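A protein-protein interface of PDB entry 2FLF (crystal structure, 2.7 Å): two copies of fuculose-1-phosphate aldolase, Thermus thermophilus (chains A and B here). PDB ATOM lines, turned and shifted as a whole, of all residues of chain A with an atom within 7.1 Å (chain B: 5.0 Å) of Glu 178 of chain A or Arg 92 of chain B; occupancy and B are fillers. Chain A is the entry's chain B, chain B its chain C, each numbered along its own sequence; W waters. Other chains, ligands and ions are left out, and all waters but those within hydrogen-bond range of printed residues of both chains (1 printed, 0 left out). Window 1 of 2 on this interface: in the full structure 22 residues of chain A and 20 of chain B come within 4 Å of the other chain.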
ATOM      1  N   GLN A  19      22.589  17.955 -17.505  1.00  0.00           N
ATOM      2  CA  GLN A  19      21.956  19.015 -16.723  1.00  0.00           C
ATOM      3  C   GLN A  19      21.452  20.166 -17.629  1.00  0.00           C
ATOM      4  O   GLN A  19      20.883  21.139 -17.155  1.00  0.00           O
ATOM      5  CB  GLN A  19      22.998  19.490 -15.696  1.00  0.00           C
ATOM      6  CG  GLN A  19      22.503  20.166 -14.443  1.00  0.00           C
ATOM      7  CD  GLN A  19      21.600  19.289 -13.601  1.00  0.00           C
ATOM      8  OE1 GLN A  19      21.553  18.078 -13.773  1.00  0.00           O
ATOM      9  NE2 GLN A  19      20.870  19.913 -12.672  1.00  0.00           N
ATOM     10  N   PRO A  91      24.089  28.291 -18.600  1.00  0.00           N
ATOM     11  CA  PRO A  91      22.889  28.039 -17.786  1.00  0.00           C
ATOM     12  C   PRO A  91      21.797  28.981 -18.291  1.00  0.00           C
ATOM     13  O   PRO A  91      21.868  30.184 -18.103  1.00  0.00           O
ATOM     14  CB  PRO A  91      23.366  28.347 -16.359  1.00  0.00           C
ATOM     15  CG  PRO A  91      24.541  29.289 -16.560  1.00  0.00           C
ATOM     16  CD  PRO A  91      25.228  28.683 -17.752  1.00  0.00           C
ATOM     17  N   VAL A  93      18.579  29.747 -17.489  1.00  0.00           N
ATOM     18  CA  VAL A  93      17.903  30.707 -16.648  1.00  0.00           C
ATOM     19  C   VAL A  93      18.856  31.789 -16.160  1.00  0.00           C
ATOM     20  O   VAL A  93      18.486  32.948 -16.116  1.00  0.00           O
ATOM     21  CB  VAL A  93      17.179  30.006 -15.499  1.00  0.00           C
ATOM     22  CG1 VAL A  93      16.643  31.025 -14.519  1.00  0.00           C
ATOM     23  CG2 VAL A  93      16.017  29.191 -16.075  1.00  0.00           C
ATOM     24  N   ASP A 108      18.930  32.157  -1.929  1.00  0.00           N
ATOM     25  CA  ASP A 108      19.135  30.898  -1.233  1.00  0.00           C
ATOM     26  C   ASP A 108      20.467  30.735  -0.521  1.00  0.00           C
ATOM     27  O   ASP A 108      21.508  31.125  -1.024  1.00  0.00           O
ATOM     28  CB  ASP A 108      18.948  29.756  -2.230  1.00  0.00           C
ATOM     29  CG  ASP A 108      19.852  29.887  -3.449  1.00  0.00           C
ATOM     30  OD1 ASP A 108      20.712  28.993  -3.620  1.00  0.00           O
ATOM     31  OD2 ASP A 108      19.700  30.871  -4.224  1.00  0.00           O
ATOM     32  N   GLU A 110      22.613  28.255  -0.052  1.00  0.00           N
ATOM     33  CA  GLU A 110      23.753  27.667  -0.756  1.00  0.00           C
ATOM     34  C   GLU A 110      24.312  28.703  -1.711  1.00  0.00           C
ATOM     35  O   GLU A 110      25.532  28.851  -1.864  1.00  0.00           O
ATOM     36  CB  GLU A 110      23.341  26.427  -1.540  1.00  0.00           C
ATOM     37  CG  GLU A 110      24.515  25.593  -2.057  1.00  0.00           C
ATOM     38  CD  GLU A 110      24.138  24.719  -3.247  1.00  0.00           C
ATOM     39  OE1 GLU A 110      24.855  23.742  -3.522  1.00  0.00           O
ATOM     40  OE2 GLU A 110      23.133  25.014  -3.921  1.00  0.00           O
ATOM     41  N   GLY A 111      23.404  29.439  -2.337  1.00  0.00           N
ATOM     42  CA  GLY A 111      23.819  30.460  -3.269  1.00  0.00           C
ATOM     43  C   GLY A 111      24.566  31.565  -2.559  1.00  0.00           C
ATOM     44  O   GLY A 111      25.500  32.146  -3.101  1.00  0.00           O
ATOM     45  N   LEU A 172      29.812  24.663  -8.885  1.00  0.00           N
ATOM     46  CA  LEU A 172      29.362  26.023  -8.666  1.00  0.00           C
ATOM     47  C   LEU A 172      28.456  26.419  -9.829  1.00  0.00           C
ATOM     48  O   LEU A 172      27.482  27.164  -9.651  1.00  0.00           O
ATOM     49  CB  LEU A 172      30.549  26.985  -8.572  1.00  0.00           C
ATOM     50  CG  LEU A 172      31.302  26.952  -7.248  1.00  0.00           C
ATOM     51  CD1 LEU A 172      32.529  27.842  -7.317  1.00  0.00           C
ATOM     52  CD2 LEU A 172      30.361  27.396  -6.153  1.00  0.00           C
ATOM     53  N   MET A 173      28.771  25.915 -11.020  1.00  0.00           N
ATOM     54  CA  MET A 173      27.959  26.225 -12.190  1.00  0.00           C
ATOM     55  C   MET A 173      26.553  25.700 -11.904  1.00  0.00           C
ATOM     56  O   MET A 173      25.539  26.340 -12.186  1.00  0.00           O
ATOM     57  CB  MET A 173      28.546  25.543 -13.423  1.00  0.00           C
ATOM     58  CG  MET A 173      27.910  25.965 -14.744  1.00  0.00           C
ATOM     59  SD  MET A 173      28.060  27.716 -15.074  1.00  0.00           S
ATOM     60  CE  MET A 173      29.718  27.926 -15.609  1.00  0.00           C
ATOM     61  N   THR A 174      26.526  24.515 -11.323  1.00  0.00           N
ATOM     62  CA  THR A 174      25.309  23.840 -10.936  1.00  0.00           C
ATOM     63  C   THR A 174      24.568  24.711  -9.906  1.00  0.00           C
ATOM     64  O   THR A 174      23.355  24.863  -9.976  1.00  0.00           O
ATOM     65  CB  THR A 174      25.719  22.459 -10.375  1.00  0.00           C
ATOM     66  OG1 THR A 174      25.438  21.449 -11.341  1.00  0.00           O
ATOM     67  CG2 THR A 174      25.068  22.154  -9.112  1.00  0.00           C
ATOM     68  N   THR A 175      25.312  25.302  -8.971  1.00  0.00           N
ATOM     69  CA  THR A 175      24.742  26.160  -7.930  1.00  0.00           C
ATOM     70  C   THR A 175      24.118  27.457  -8.460  1.00  0.00           C
ATOM     71  O   THR A 175      23.107  27.917  -7.949  1.00  0.00           O
ATOM     72  CB  THR A 175      25.808  26.571  -6.899  1.00  0.00           C
ATOM     73  OG1 THR A 175      26.387  25.401  -6.304  1.00  0.00           O
ATOM     74  CG2 THR A 175      25.183  27.451  -5.811  1.00  0.00           C
ATOM     75  N   LEU A 176      24.749  28.054  -9.466  1.00  0.00           N
ATOM     76  CA  LEU A 176      24.244  29.279 -10.047  1.00  0.00           C
ATOM     77  C   LEU A 176      22.872  29.065 -10.671  1.00  0.00           C
ATOM     78  O   LEU A 176      21.955  29.862 -10.424  1.00  0.00           O
ATOM     79  CB  LEU A 176      25.227  29.789 -11.096  1.00  0.00           C
ATOM     80  CG  LEU A 176      24.897  31.004 -11.971  1.00  0.00           C
ATOM     81  CD1 LEU A 176      24.686  32.254 -11.138  1.00  0.00           C
ATOM     82  CD2 LEU A 176      26.050  31.199 -12.951  1.00  0.00           C
ATOM     83  N   GLU A 177      22.727  27.989 -11.461  1.00  0.00           N
ATOM     84  CA  GLU A 177      21.451  27.701 -12.127  1.00  0.00           C
ATOM     85  C   GLU A 177      20.319  27.408 -11.167  1.00  0.00           C
ATOM     86  O   GLU A 177      19.166  27.724 -11.455  1.00  0.00           O
ATOM     87  CB  GLU A 177      21.565  26.527 -13.111  1.00  0.00           C
ATOM     88  CG  GLU A 177      21.577  26.936 -14.579  1.00  0.00           C
ATOM     89  CD  GLU A 177      20.337  27.707 -15.045  1.00  0.00           C
ATOM     90  OE1 GLU A 177      19.325  27.061 -15.369  1.00  0.00           O
ATOM     91  OE2 GLU A 177      20.370  28.953 -15.100  1.00  0.00           O
ATOM     92  N   GLU A 178      20.644  26.775 -10.047  1.00  0.00           N
ATOM     93  CA  GLU A 178      19.636  26.464  -9.031  1.00  0.00           C
ATOM     94  C   GLU A 178      19.120  27.845  -8.596  1.00  0.00           C
ATOM     95  O   GLU A 178      17.917  28.104  -8.631  1.00  0.00           O
ATOM     96  CB  GLU A 178      20.306  25.707  -7.866  1.00  0.00           C
ATOM     97  CG  GLU A 178      19.425  25.190  -6.716  1.00  0.00           C
ATOM     98  CD  GLU A 178      20.259  24.486  -5.614  1.00  0.00           C
ATOM     99  OE1 GLU A 178      21.214  25.112  -5.095  1.00  0.00           O
ATOM    100  OE2 GLU A 178      19.968  23.315  -5.264  1.00  0.00           O
ATOM    101  N   SER A 179      20.062  28.736  -8.261  1.00  0.00           N
ATOM    102  CA  SER A 179      19.780  30.085  -7.817  1.00  0.00           C
ATOM    103  C   SER A 179      18.987  30.960  -8.785  1.00  0.00           C
ATOM    104  O   SER A 179      18.027  31.640  -8.386  1.00  0.00           O
ATOM    105  CB  SER A 179      21.077  30.799  -7.466  1.00  0.00           C
ATOM    106  OG  SER A 179      21.590  30.406  -6.214  1.00  0.00           O
ATOM    107  N   ALA A 180      19.386  30.965 -10.049  1.00  0.00           N
ATOM    108  CA  ALA A 180      18.694  31.804 -11.017  1.00  0.00           C
ATOM    109  C   ALA A 180      17.246  31.375 -11.087  1.00  0.00           C
ATOM    110  O   ALA A 180      16.328  32.191 -11.259  1.00  0.00           O
ATOM    111  CB  ALA A 180      19.344  31.693 -12.383  1.00  0.00           C
ATOM    112  N   GLN A 181      17.056  30.072 -10.953  1.00  0.00           N
ATOM    113  CA  GLN A 181      15.727  29.503 -10.988  1.00  0.00           C
ATOM    114  C   GLN A 181      14.976  29.921  -9.734  1.00  0.00           C
ATOM    115  O   GLN A 181      13.835  30.360  -9.820  1.00  0.00           O
ATOM    116  CB  GLN A 181      15.815  27.980 -11.116  1.00  0.00           C
ATOM    117  CG  GLN A 181      16.452  27.557 -12.433  1.00  0.00           C
ATOM    118  CD  GLN A 181      16.181  26.118 -12.778  1.00  0.00           C
ATOM    119  OE1 GLN A 181      15.207  25.534 -12.324  1.00  0.00           O
ATOM    120  NE2 GLN A 181      17.030  25.545 -13.601  1.00  0.00           N
ATOM    121  N   ILE A 182      15.617  29.822  -8.570  1.00  0.00           N
ATOM    122  CA  ILE A 182      14.945  30.223  -7.337  1.00  0.00           C
ATOM    123  C   ILE A 182      14.539  31.686  -7.475  1.00  0.00           C
ATOM    124  O   ILE A 182      13.435  32.081  -7.115  1.00  0.00           O
ATOM    125  CB  ILE A 182      15.843  30.042  -6.131  1.00  0.00           C
ATOM    126  CG1 ILE A 182      16.232  28.570  -6.011  1.00  0.00           C
ATOM    127  CG2 ILE A 182      15.113  30.517  -4.871  1.00  0.00           C
ATOM    128  CD1 ILE A 182      16.341  28.074  -4.600  1.00  0.00           C
ATOM    129  N   LEU A 183      15.448  32.472  -8.034  1.00  0.00           N
ATOM    130  CA  LEU A 183      15.198  33.869  -8.281  1.00  0.00           C
ATOM    131  C   LEU A 183      13.995  33.956  -9.206  1.00  0.00           C
ATOM    132  O   LEU A 183      12.956  34.474  -8.825  1.00  0.00           O
ATOM    133  CB  LEU A 183      16.425  34.513  -8.929  1.00  0.00           C
ATOM    134  CG  LEU A 183      17.609  34.834  -8.013  1.00  0.00           C
ATOM    135  CD1 LEU A 183      18.818  35.283  -8.825  1.00  0.00           C
ATOM    136  CD2 LEU A 183      17.183  35.897  -7.059  1.00  0.00           C
ATOM    137  N   LEU A 184      14.120  33.419 -10.412  1.00  0.00           N
ATOM    138  CA  LEU A 184      13.022  33.469 -11.375  1.00  0.00           C
ATOM    139  C   LEU A 184      11.637  33.173 -10.783  1.00  0.00           C
ATOM    140  O   LEU A 184      10.735  34.005 -10.889  1.00  0.00           O
ATOM    141  CB  LEU A 184      13.297  32.527 -12.543  1.00  0.00           C
ATOM    142  CG  LEU A 184      12.245  32.528 -13.652  1.00  0.00           C
ATOM    143  CD1 LEU A 184      12.068  33.935 -14.162  1.00  0.00           C
ATOM    144  CD2 LEU A 184      12.662  31.594 -14.777  1.00  0.00           C
ATOM    145  N   TYR A 185      11.477  32.000 -10.166  1.00  0.00           N
ATOM    146  CA  TYR A 185      10.204  31.598  -9.563  1.00  0.00           C
ATOM    147  C   TYR A 185       9.806  32.549  -8.431  1.00  0.00           C
ATOM    148  O   TYR A 185       8.673  33.009  -8.375  1.00  0.00           O
ATOM    149  CB  TYR A 185      10.282  30.160  -9.024  1.00  0.00           C
ATOM    150  CG  TYR A 185      10.727  29.136 -10.052  1.00  0.00           C
ATOM    151  CD1 TYR A 185      11.703  28.199  -9.746  1.00  0.00           C
ATOM    152  CD2 TYR A 185      10.200  29.134 -11.337  1.00  0.00           C
ATOM    153  CE1 TYR A 185      12.147  27.297 -10.686  1.00  0.00           C
ATOM    154  CE2 TYR A 185      10.631  28.232 -12.286  1.00  0.00           C
ATOM    155  CZ  TYR A 185      11.607  27.317 -11.948  1.00  0.00           C
ATOM    156  OH  TYR A 185      12.039  26.408 -12.875  1.00  0.00           O
ATOM    157  N   HIS A 186      10.724  32.851  -7.527  1.00  0.00           N
ATOM    158  CA  HIS A 186      10.387  33.774  -6.458  1.00  0.00           C
ATOM    159  C   HIS A 186       9.725  35.018  -7.055  1.00  0.00           C
ATOM    160  O   HIS A 186       8.609  35.388  -6.685  1.00  0.00           O
ATOM    161  CB  HIS A 186      11.640  34.181  -5.699  1.00  0.00           C
ATOM    162  CG  HIS A 186      11.387  35.152  -4.588  1.00  0.00           C
ATOM    163  ND1 HIS A 186      11.523  36.513  -4.744  1.00  0.00           N
ATOM    164  CD2 HIS A 186      11.005  34.957  -3.304  1.00  0.00           C
ATOM    165  CE1 HIS A 186      11.238  37.113  -3.603  1.00  0.00           C
ATOM    166  NE2 HIS A 186      10.921  36.193  -2.712  1.00  0.00           N
ATOM    167  N   GLY B  20      16.217  17.838 -10.865  1.00  0.00           N
ATOM    168  CA  GLY B  20      16.420  19.260 -10.646  1.00  0.00           C
ATOM    169  C   GLY B  20      16.211  19.681  -9.199  1.00  0.00           C
ATOM    170  O   GLY B  20      16.104  20.850  -8.894  1.00  0.00           O
ATOM    171  N   LEU B  21      16.180  18.707  -8.306  1.00  0.00           N
ATOM    172  CA  LEU B  21      15.955  18.948  -6.904  1.00  0.00           C
ATOM    173  C   LEU B  21      17.223  19.094  -6.076  1.00  0.00           C
ATOM    174  O   LEU B  21      17.141  19.198  -4.864  1.00  0.00           O
ATOM    175  CB  LEU B  21      15.099  17.816  -6.340  1.00  0.00           C
ATOM    176  CG  LEU B  21      13.799  17.564  -7.095  1.00  0.00           C
ATOM    177  CD1 LEU B  21      13.204  16.281  -6.579  1.00  0.00           C
ATOM    178  CD2 LEU B  21      12.823  18.735  -6.899  1.00  0.00           C
ATOM    179  N   ILE B  22      18.391  19.073  -6.712  1.00  0.00           N
ATOM    180  CA  ILE B  22      19.640  19.271  -5.989  1.00  0.00           C
ATOM    181  C   ILE B  22      20.742  19.624  -6.962  1.00  0.00           C
ATOM    182  O   ILE B  22      20.683  19.256  -8.139  1.00  0.00           O
ATOM    183  CB  ILE B  22      20.148  18.019  -5.213  1.00  0.00           C
ATOM    184  CG1 ILE B  22      20.354  16.864  -6.178  1.00  0.00           C
ATOM    185  CG2 ILE B  22      19.187  17.611  -4.112  1.00  0.00           C
ATOM    186  CD1 ILE B  22      21.025  15.700  -5.525  1.00  0.00           C
ATOM    187  N   SER B  23      21.729  20.354  -6.454  1.00  0.00           N
ATOM    188  CA  SER B  23      22.909  20.741  -7.190  1.00  0.00           C
ATOM    189  C   SER B  23      23.759  19.481  -7.235  1.00  0.00           C
ATOM    190  O   SER B  23      23.445  18.489  -6.581  1.00  0.00           O
ATOM    191  CB  SER B  23      23.699  21.806  -6.421  1.00  0.00           C
ATOM    192  OG  SER B  23      23.169  23.091  -6.650  1.00  0.00           O
ATOM    193  N   ALA B  26      24.642  19.312  -3.315  1.00  0.00           N
ATOM    194  CA  ALA B  26      23.783  19.732  -2.220  1.00  0.00           C
ATOM    195  C   ALA B  26      22.929  18.564  -1.752  1.00  0.00           C
ATOM    196  O   ALA B  26      22.966  17.475  -2.316  1.00  0.00           O
ATOM    197  CB  ALA B  26      22.876  20.880  -2.663  1.00  0.00           C
ATOM    198  N   HIS B  90      16.507  20.209  -2.423  1.00  0.00           N
ATOM    199  CA  HIS B  90      16.260  21.612  -2.618  1.00  0.00           C
ATOM    200  C   HIS B  90      15.310  21.888  -3.764  1.00  0.00           C
ATOM    201  O   HIS B  90      15.738  22.287  -4.841  1.00  0.00           O
ATOM    202  CB  HIS B  90      17.569  22.370  -2.829  1.00  0.00           C
ATOM    203  CG  HIS B  90      18.488  22.337  -1.644  1.00  0.00           C
ATOM    204  ND1 HIS B  90      19.327  21.276  -1.377  1.00  0.00           N
ATOM    205  CD2 HIS B  90      18.679  23.225  -0.642  1.00  0.00           C
ATOM    206  CE1 HIS B  90      19.996  21.511  -0.261  1.00  0.00           C
ATOM    207  NE2 HIS B  90      19.620  22.687   0.205  1.00  0.00           N
ATOM    208  N   PRO B  91      14.000  21.634  -3.556  1.00  0.00           N
ATOM    209  CA  PRO B  91      12.966  21.876  -4.573  1.00  0.00           C
ATOM    210  C   PRO B  91      12.974  23.372  -4.857  1.00  0.00           C
ATOM    211  O   PRO B  91      12.845  24.185  -3.948  1.00  0.00           O
ATOM    212  CB  PRO B  91      11.688  21.423  -3.888  1.00  0.00           C
ATOM    213  CG  PRO B  91      12.028  21.527  -2.426  1.00  0.00           C
ATOM    214  CD  PRO B  91      13.410  21.006  -2.366  1.00  0.00           C
ATOM    215  N   ARG B  92      13.141  23.735  -6.115  1.00  0.00           N
ATOM    216  CA  ARG B  92      13.219  25.126  -6.457  1.00  0.00           C
ATOM    217  C   ARG B  92      11.942  25.908  -6.356  1.00  0.00           C
ATOM    218  O   ARG B  92      11.879  26.869  -5.594  1.00  0.00           O
ATOM    219  CB  ARG B  92      13.854  25.269  -7.825  1.00  0.00           C
ATOM    220  CG  ARG B  92      15.311  24.897  -7.738  1.00  0.00           C
ATOM    221  CD  ARG B  92      15.757  24.095  -8.919  1.00  0.00           C
ATOM    222  NE  ARG B  92      17.039  23.461  -8.654  1.00  0.00           N
ATOM    223  CZ  ARG B  92      17.943  23.253  -9.593  1.00  0.00           C
ATOM    224  NH1 ARG B  92      17.674  23.644 -10.830  1.00  0.00           N
ATOM    225  NH2 ARG B  92      19.102  22.665  -9.298  1.00  0.00           N
ATOM    226  N   VAL B  93      10.922  25.534  -7.110  1.00  0.00           N
ATOM    227  CA  VAL B  93       9.671  26.258  -7.010  1.00  0.00           C
ATOM    228  C   VAL B  93       9.232  26.328  -5.551  1.00  0.00           C
ATOM    229  O   VAL B  93       8.761  27.366  -5.076  1.00  0.00           O
ATOM    230  CB  VAL B  93       8.599  25.575  -7.801  1.00  0.00           C
ATOM    231  CG1 VAL B  93       7.274  26.282  -7.616  1.00  0.00           C
ATOM    232  CG2 VAL B  93       9.010  25.568  -9.251  1.00  0.00           C
ATOM    233  N   ALA B  94       9.422  25.226  -4.837  1.00  0.00           N
ATOM    234  CA  ALA B  94       9.029  25.155  -3.443  1.00  0.00           C
ATOM    235  C   ALA B  94       9.795  26.116  -2.529  1.00  0.00           C
ATOM    236  O   ALA B  94       9.211  26.698  -1.630  1.00  0.00           O
ATOM    237  CB  ALA B  94       9.180  23.747  -2.952  1.00  0.00           C
ATOM    238  N   VAL B  95      11.102  26.264  -2.736  1.00  0.00           N
ATOM    239  CA  VAL B  95      11.883  27.180  -1.913  1.00  0.00           C
ATOM    240  C   VAL B  95      11.456  28.622  -2.189  1.00  0.00           C
ATOM    241  O   VAL B  95      11.304  29.432  -1.279  1.00  0.00           O
ATOM    242  CB  VAL B  95      13.389  27.032  -2.185  1.00  0.00           C
ATOM    243  CG1 VAL B  95      14.107  28.312  -1.863  1.00  0.00           C
ATOM    244  CG2 VAL B  95      13.951  25.925  -1.345  1.00  0.00           C
ATOM    245  N   ALA B  96      11.245  28.926  -3.456  1.00  0.00           N
ATOM    246  CA  ALA B  96      10.827  30.249  -3.859  1.00  0.00           C
ATOM    247  C   ALA B  96       9.501  30.651  -3.211  1.00  0.00           C
ATOM    248  O   ALA B  96       9.356  31.779  -2.760  1.00  0.00           O
ATOM    249  CB  ALA B  96      10.723  30.319  -5.374  1.00  0.00           C
ATOM    250  N   GLU B 177       7.466  19.129  -4.695  1.00  0.00           N
ATOM    251  CA  GLU B 177       7.839  20.008  -5.793  1.00  0.00           C
ATOM    252  C   GLU B 177       6.775  20.112  -6.869  1.00  0.00           C
ATOM    253  O   GLU B 177       6.655  21.130  -7.534  1.00  0.00           O
ATOM    254  CB  GLU B 177       9.161  19.555  -6.420  1.00  0.00           C
ATOM    255  CG  GLU B 177       9.648  20.476  -7.521  1.00  0.00           C
ATOM    256  CD  GLU B 177       9.895  21.925  -7.061  1.00  0.00           C
ATOM    257  OE1 GLU B 177      10.385  22.721  -7.888  1.00  0.00           O
ATOM    258  OE2 GLU B 177       9.603  22.273  -5.896  1.00  0.00           O
HETATM  259  O   HOH W   1      21.785  20.754 -10.564  1.00  0.00           O
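Of chain B, only Ser 23, His 90 and Arg 92 come within 4 Å of Glu 178 of chain A.
Of the printed residues of chain A, Arg 92 of chain B touches Glu 178, Gln 181 and Tyr 185.
Of the printed residues of chain B, Ile 182 of chain A touches Val 95 (3.5 Å) and Ala 96 (3.7 Å).
Of the printed residues of chain B, His 186 of chain A touches Ala 96.
Printed residues of chain A within 4 Å of Ser 23 of chain B: Glu 110 (3.3 Å), Thr 174 (3.0 Å), Thr 175 (3.7 Å) and Glu 178 (3.2 Å).
Printed residues of chain A within 4 Å of Ala 26 of chain B: Glu 110 (3.6 Å).
Ser 179 of chain A touches none of the printed residues of chain B.
Pro 91 of chain B touches none of the printed residues of chain A.
The nearest residue of chain B that does not touch Glu 178 of chain A is Ile 22 of chain B (4.1 Å).
The nearest printed residue of chain B that does not touch His 186 of chain A is Val 95 of chain B (5.9 Å).
Hydrophobic or aromatic side chains of chain A within 4 Å of the printed part of chain B: Ile 182, Tyr 185 and His 186.
Of the 13 printed residues of chain B, 7 touch a printed residue of chain A.
Among the printed residues, 14 pairs touch across the chains.
Among the printed residues, no Asp or Glu carboxylate lies within 4 Å of a Lys or Arg side-chain nitrogen of the other chain.
3 positions are printed for both chains.
Of the 14 pairs that touch across the chains among the printed residues, none has its exchanged pair printed and touching as well.
Water W1 lies within hydrogen-bond range of NE2 of Gln 19 of chain A (2.4 Å) and O of Ile 22 of chain B (3.1 Å).
The side-chain carboxylate of Glu 110 of chain A is in hydrogen-bond range of the side-chain hydroxyl of Ser 23 of chain B.
OE1 of Glu 178 of chain A sits at hydrogen-bond distance from OG of Ser 23 of chain B (3.2 Å).
The side-chain amide nitrogen of Gln 181 of chain A sits close to the guanidinium group of Arg 92 of chain B.
Among the printed residues, merely in contact across the chains: Thr 174 of chain A with Ser 23 of chain B, His 186 of chain A with Ala 96 of chain B, Glu 178 of chain A with Arg 92 of chain B, Ile 182 of chain A with Val 95 of chain B, Glu 178 of chain A with His 90 of chain B, Glu 110 of chain A with Ala 26 of chain B, Ile 182 of chain A with Ala 96 of chain B, Thr 175 of chain A with Ser 23 of chain B, Tyr 185 of chain A with Ala 96 of chain B, Tyr 185 of chain A with Val 93 of chain B and Tyr 185 of chain A with Arg 92 of chain B.
O of Thr 175 of chain A lies within hydrogen-bond range of OG of Ser 179 of chain A, 3.4 Å away.
OE1 of Glu 177 of chain A lies within hydrogen-bond range of NE2 of Gln 181 of chain A (3.3 Å).
OE1 of Gln 181 of chain A sits at hydrogen-bond distance from OH of Tyr 185 of chain A.
The backbone carbonyl oxygen (O) of Gly 20 of chain B sits at hydrogen-bond distance from the guanidinium group (NE) of Arg 92 of chain B (2.8 Å).
The backbone carbonyl oxygen of Leu 21 of chain B is in hydrogen-bond range of the backbone NH of His 90 of chain B, 2.7 Å away.
The backbone NH (N) of Val 93 of chain B sits at hydrogen-bond distance from the side-chain carboxylate (OE1) of Glu 177 of chain B (3.0 Å).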
